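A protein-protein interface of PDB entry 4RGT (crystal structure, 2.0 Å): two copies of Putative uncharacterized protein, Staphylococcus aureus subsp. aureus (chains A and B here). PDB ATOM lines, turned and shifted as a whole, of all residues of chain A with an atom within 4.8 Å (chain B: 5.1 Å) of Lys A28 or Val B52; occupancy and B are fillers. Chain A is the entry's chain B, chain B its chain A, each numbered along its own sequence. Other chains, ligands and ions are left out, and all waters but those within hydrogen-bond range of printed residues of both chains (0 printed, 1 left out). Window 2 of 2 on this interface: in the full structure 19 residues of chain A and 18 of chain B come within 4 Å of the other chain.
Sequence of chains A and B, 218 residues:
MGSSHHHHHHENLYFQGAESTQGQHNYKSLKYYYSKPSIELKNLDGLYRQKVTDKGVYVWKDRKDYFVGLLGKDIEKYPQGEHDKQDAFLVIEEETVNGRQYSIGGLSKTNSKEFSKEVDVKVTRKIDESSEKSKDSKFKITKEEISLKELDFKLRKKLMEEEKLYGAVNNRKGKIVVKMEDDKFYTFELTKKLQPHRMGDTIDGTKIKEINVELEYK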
ATOM      1  N   ASN A  26     -27.229   0.377 -22.703  1.00  0.00           N
ATOM      2  CA  ASN A  26     -25.926   0.968 -22.398  1.00  0.00           C
ATOM      3  C   ASN A  26     -25.281   0.343 -21.148  1.00  0.00           C
ATOM      4  O   ASN A  26     -25.828   0.426 -20.045  1.00  0.00           O
ATOM      5  CB  ASN A  26     -26.084   2.486 -22.233  1.00  0.00           C
ATOM      6  CG  ASN A  26     -24.762   3.206 -22.082  1.00  0.00           C
ATOM      7  OD1 ASN A  26     -24.543   3.916 -21.100  1.00  0.00           O
ATOM      8  ND2 ASN A  26     -23.863   3.024 -23.056  1.00  0.00           N
ATOM      9  N   TYR A  27     -24.126  -0.293 -21.330  1.00  0.00           N
ATOM     10  CA  TYR A  27     -23.419  -0.917 -20.206  1.00  0.00           C
ATOM     11  C   TYR A  27     -22.921   0.122 -19.200  1.00  0.00           C
ATOM     12  O   TYR A  27     -23.001  -0.092 -17.989  1.00  0.00           O
ATOM     13  CB  TYR A  27     -22.256  -1.767 -20.688  1.00  0.00           C
ATOM     14  CG  TYR A  27     -21.428  -2.328 -19.553  1.00  0.00           C
ATOM     15  CD1 TYR A  27     -21.790  -3.508 -18.927  1.00  0.00           C
ATOM     16  CD2 TYR A  27     -20.284  -1.668 -19.108  1.00  0.00           C
ATOM     17  CE1 TYR A  27     -21.043  -4.018 -17.891  1.00  0.00           C
ATOM     18  CE2 TYR A  27     -19.527  -2.174 -18.071  1.00  0.00           C
ATOM     19  CZ  TYR A  27     -19.908  -3.351 -17.473  1.00  0.00           C
ATOM     20  OH  TYR A  27     -19.165  -3.869 -16.443  1.00  0.00           O
ATOM     21  N   LYS A  28     -22.413   1.242 -19.708  1.00  0.00           N
ATOM     22  CA  LYS A  28     -21.929   2.323 -18.855  1.00  0.00           C
ATOM     23  C   LYS A  28     -23.036   2.829 -17.898  1.00  0.00           C
ATOM     24  O   LYS A  28     -22.816   2.945 -16.695  1.00  0.00           O
ATOM     25  CB  LYS A  28     -21.379   3.469 -19.716  1.00  0.00           C
ATOM     26  CG  LYS A  28     -20.784   4.645 -18.949  1.00  0.00           C
ATOM     27  CD  LYS A  28     -20.116   5.622 -19.917  1.00  0.00           C
ATOM     28  CE  LYS A  28     -19.536   6.838 -19.214  1.00  0.00           C
ATOM     29  NZ  LYS A  28     -20.547   7.708 -18.565  1.00  0.00           N
ATOM     30  N   SER A  29     -24.229   3.093 -18.427  1.00  0.00           N
ATOM     31  CA  SER A  29     -25.315   3.643 -17.611  1.00  0.00           C
ATOM     32  C   SER A  29     -25.886   2.577 -16.674  1.00  0.00           C
ATOM     33  O   SER A  29     -26.324   2.892 -15.575  1.00  0.00           O
ATOM     34  CB  SER A  29     -26.399   4.252 -18.498  1.00  0.00           C
ATOM     35  OG  SER A  29     -27.183   5.178 -17.773  1.00  0.00           O
ATOM     36  N   LEU A  30     -25.871   1.324 -17.133  1.00  0.00           N
ATOM     37  CA  LEU A  30     -26.285   0.163 -16.347  1.00  0.00           C
ATOM     38  C   LEU A  30     -25.403   0.050 -15.088  1.00  0.00           C
ATOM     39  O   LEU A  30     -25.897   0.068 -13.939  1.00  0.00           O
ATOM     40  CB  LEU A  30     -26.162  -1.116 -17.203  1.00  0.00           C
ATOM     41  CG  LEU A  30     -26.443  -2.490 -16.567  1.00  0.00           C
ATOM     42  CD1 LEU A  30     -27.874  -2.590 -16.047  1.00  0.00           C
ATOM     43  CD2 LEU A  30     -26.195  -3.622 -17.552  1.00  0.00           C
ATOM     44  N   LYS A  31     -24.097  -0.035 -15.309  1.00  0.00           N
ATOM     45  CA  LYS A  31     -23.148  -0.158 -14.199  1.00  0.00           C
ATOM     46  C   LYS A  31     -23.127   1.102 -13.336  1.00  0.00           C
ATOM     47  O   LYS A  31     -22.989   1.041 -12.120  1.00  0.00           O
ATOM     48  CB  LYS A  31     -21.742  -0.430 -14.736  1.00  0.00           C
ATOM     49  CG  LYS A  31     -20.669  -0.570 -13.672  1.00  0.00           C
ATOM     50  CD  LYS A  31     -21.008  -1.676 -12.680  1.00  0.00           C
ATOM     51  CE  LYS A  31     -19.841  -1.981 -11.742  1.00  0.00           C
ATOM     52  NZ  LYS A  31     -18.621  -2.461 -12.452  1.00  0.00           N
ATOM     53  N   TYR A  32     -23.257   2.256 -13.968  1.00  0.00           N
ATOM     54  CA  TYR A  32     -23.224   3.501 -13.219  1.00  0.00           C
ATOM     55  C   TYR A  32     -24.340   3.478 -12.189  1.00  0.00           C
ATOM     56  O   TYR A  32     -24.136   3.836 -11.012  1.00  0.00           O
ATOM     57  CB  TYR A  32     -23.375   4.695 -14.159  1.00  0.00           C
ATOM     58  CG  TYR A  32     -23.062   6.014 -13.509  1.00  0.00           C
ATOM     59  CD1 TYR A  32     -21.749   6.358 -13.200  1.00  0.00           C
ATOM     60  CD2 TYR A  32     -24.062   6.934 -13.235  1.00  0.00           C
ATOM     61  CE1 TYR A  32     -21.448   7.577 -12.616  1.00  0.00           C
ATOM     62  CE2 TYR A  32     -23.767   8.154 -12.655  1.00  0.00           C
ATOM     63  CZ  TYR A  32     -22.467   8.473 -12.346  1.00  0.00           C
ATOM     64  OH  TYR A  32     -22.183   9.688 -11.767  1.00  0.00           O
ATOM     65  N   ARG B  49     -26.900  15.901 -26.005  1.00  0.00           N
ATOM     66  CA  ARG B  49     -26.827  14.860 -24.987  1.00  0.00           C
ATOM     67  C   ARG B  49     -25.524  15.129 -24.260  1.00  0.00           C
ATOM     68  O   ARG B  49     -24.449  14.816 -24.787  1.00  0.00           O
ATOM     69  CB  ARG B  49     -26.761  13.496 -25.655  1.00  0.00           C
ATOM     70  CG  ARG B  49     -26.740  12.327 -24.703  1.00  0.00           C
ATOM     71  CD  ARG B  49     -28.129  12.039 -24.159  1.00  0.00           C
ATOM     72  NE  ARG B  49     -28.100  10.996 -23.139  1.00  0.00           N
ATOM     73  CZ  ARG B  49     -28.119   9.691 -23.380  1.00  0.00           C
ATOM     74  NH1 ARG B  49     -28.165   9.226 -24.614  1.00  0.00           N
ATOM     75  NH2 ARG B  49     -28.093   8.838 -22.370  1.00  0.00           N
ATOM     76  N   GLN B  50     -25.600  15.727 -23.076  1.00  0.00           N
ATOM     77  CA  GLN B  50     -24.399  16.078 -22.334  1.00  0.00           C
ATOM     78  C   GLN B  50     -23.542  14.861 -21.976  1.00  0.00           C
ATOM     79  O   GLN B  50     -22.317  14.905 -22.126  1.00  0.00           O
ATOM     80  CB  GLN B  50     -24.707  16.943 -21.103  1.00  0.00           C
ATOM     81  CG  GLN B  50     -23.434  17.571 -20.528  1.00  0.00           C
ATOM     82  CD  GLN B  50     -23.663  18.759 -19.595  1.00  0.00           C
ATOM     83  OE1 GLN B  50     -24.658  18.837 -18.882  1.00  0.00           O
ATOM     84  NE2 GLN B  50     -22.711  19.684 -19.586  1.00  0.00           N
ATOM     85  N   LYS B  51     -24.179  13.787 -21.518  1.00  0.00           N
ATOM     86  CA  LYS B  51     -23.465  12.542 -21.190  1.00  0.00           C
ATOM     87  C   LYS B  51     -24.397  11.340 -21.262  1.00  0.00           C
ATOM     88  O   LYS B  51     -25.617  11.485 -21.116  1.00  0.00           O
ATOM     89  CB  LYS B  51     -22.711  12.640 -19.847  1.00  0.00           C
ATOM     90  CG  LYS B  51     -23.417  13.378 -18.723  1.00  0.00           C
ATOM     91  CD  LYS B  51     -22.496  13.472 -17.507  1.00  0.00           C
ATOM     92  CE  LYS B  51     -22.987  14.482 -16.479  1.00  0.00           C
ATOM     93  NZ  LYS B  51     -24.380  14.191 -16.030  1.00  0.00           N
ATOM     94  N   VAL B  52     -23.835  10.162 -21.551  1.00  0.00           N
ATOM     95  CA  VAL B  52     -24.654   8.969 -21.711  1.00  0.00           C
ATOM     96  C   VAL B  52     -25.320   8.555 -20.404  1.00  0.00           C
ATOM     97  O   VAL B  52     -26.228   7.728 -20.416  1.00  0.00           O
ATOM     98  CB  VAL B  52     -23.899   7.751 -22.298  1.00  0.00           C
ATOM     99  CG1 VAL B  52     -23.416   8.027 -23.722  1.00  0.00           C
ATOM    100  CG2 VAL B  52     -22.754   7.321 -21.402  1.00  0.00           C
ATOM    101  N   THR B  53     -24.856   9.092 -19.278  1.00  0.00           N
ATOM    102  CA  THR B  53     -25.509   8.814 -18.005  1.00  0.00           C
ATOM    103  C   THR B  53     -26.745   9.729 -17.791  1.00  0.00           C
ATOM    104  O   THR B  53     -27.518   9.516 -16.859  1.00  0.00           O
ATOM    105  CB  THR B  53     -24.533   8.912 -16.826  1.00  0.00           C
ATOM    106  OG1 THR B  53     -23.906  10.185 -16.838  1.00  0.00           O
ATOM    107  CG2 THR B  53     -23.480   7.841 -16.928  1.00  0.00           C
ATOM    108  N   ASP B  54     -26.926  10.740 -18.640  1.00  0.00           N
ATOM    109  CA  ASP B  54     -28.119  11.583 -18.577  1.00  0.00           C
ATOM    110  C   ASP B  54     -29.295  10.854 -19.247  1.00  0.00           C
ATOM    111  O   ASP B  54     -29.144  10.302 -20.341  1.00  0.00           O
ATOM    112  CB  ASP B  54     -27.929  12.893 -19.327  1.00  0.00           C
ATOM    113  CG  ASP B  54     -27.087  13.888 -18.586  1.00  0.00           C
ATOM    114  OD1 ASP B  54     -26.660  13.628 -17.434  1.00  0.00           O
ATOM    115  OD2 ASP B  54     -26.859  14.965 -19.165  1.00  0.00           O
ATOM    116  N   PRO B  79     -26.518   9.372 -28.811  1.00  0.00           N
ATOM    117  CA  PRO B  79     -25.277   9.228 -28.029  1.00  0.00           C
ATOM    118  C   PRO B  79     -24.743  10.589 -27.627  1.00  0.00           C
ATOM    119  O   PRO B  79     -25.270  11.613 -28.075  1.00  0.00           O
ATOM    120  CB  PRO B  79     -24.314   8.515 -28.992  1.00  0.00           C
ATOM    121  CG  PRO B  79     -24.931   8.637 -30.352  1.00  0.00           C
ATOM    122  CD  PRO B  79     -26.414   8.709 -30.125  1.00  0.00           C
ATOM    123  N   GLN B  80     -23.695  10.607 -26.815  1.00  0.00           N
ATOM    124  CA  GLN B  80     -23.127  11.855 -26.306  1.00  0.00           C
ATOM    125  C   GLN B  80     -22.774  12.814 -27.448  1.00  0.00           C
ATOM    126  O   GLN B  80     -22.199  12.398 -28.444  1.00  0.00           O
ATOM    127  CB  GLN B  80     -21.867  11.538 -25.491  1.00  0.00           C
ATOM    128  CG  GLN B  80     -21.372  12.656 -24.569  1.00  0.00           C
ATOM    129  CD  GLN B  80     -20.740  13.817 -25.290  1.00  0.00           C
ATOM    130  OE1 GLN B  80     -20.080  13.642 -26.310  1.00  0.00           O
ATOM    131  NE2 GLN B  80     -20.915  15.018 -24.746  1.00  0.00           N
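Of the printed residues of chain B, Lys A28 touches Val B52 (3.5 Å) and Thr B53 (3.4 Å).
Printed residues of chain A within 4 Å of Val B52: Asn A26, Lys A28 and Ser A29.
Printed residues of chain B within 4 Å of Asn A26: Val B52 (3.9 Å).
Of the printed residues of chain B, Tyr A32 touches Thr B53 (3.8 Å).
Of the printed residues of chain B, Ser A29 touches Val B52.
Of the printed residues of chain A, Thr B53 touches Lys A28 and Tyr A32.
Gln B50 touches none of the printed residues of chain A.
The nearest printed residue of chain A that does not touch Val B52 is Leu A30 (7.2 Å).
No position is printed for both chains.
The side-chain amide oxygen of Asn A26 sits at hydrogen-bond distance from the backbone NH of Ser A29.
NH2 of Arg B49 is in hydrogen-bond range of O of Val B52, at 2.9 Å.
Among the printed residues, merely in contact across the chains: Asn A26 with Val B52, Lys A28 with Val B52, Lys A28 with Thr B53, Ser A29 with Val B52 and Tyr A32 with Thr B53.
Printed residues of chain B that touch a printed residue of chain A: Val B52 and Thr B53.
Hydrophobic or aromatic side chains of chain B within 4 Å of the printed part of chain A: Val B52.
Hydrophobic or aromatic side chains of chain A that line the printed part of chain B: Tyr A32.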
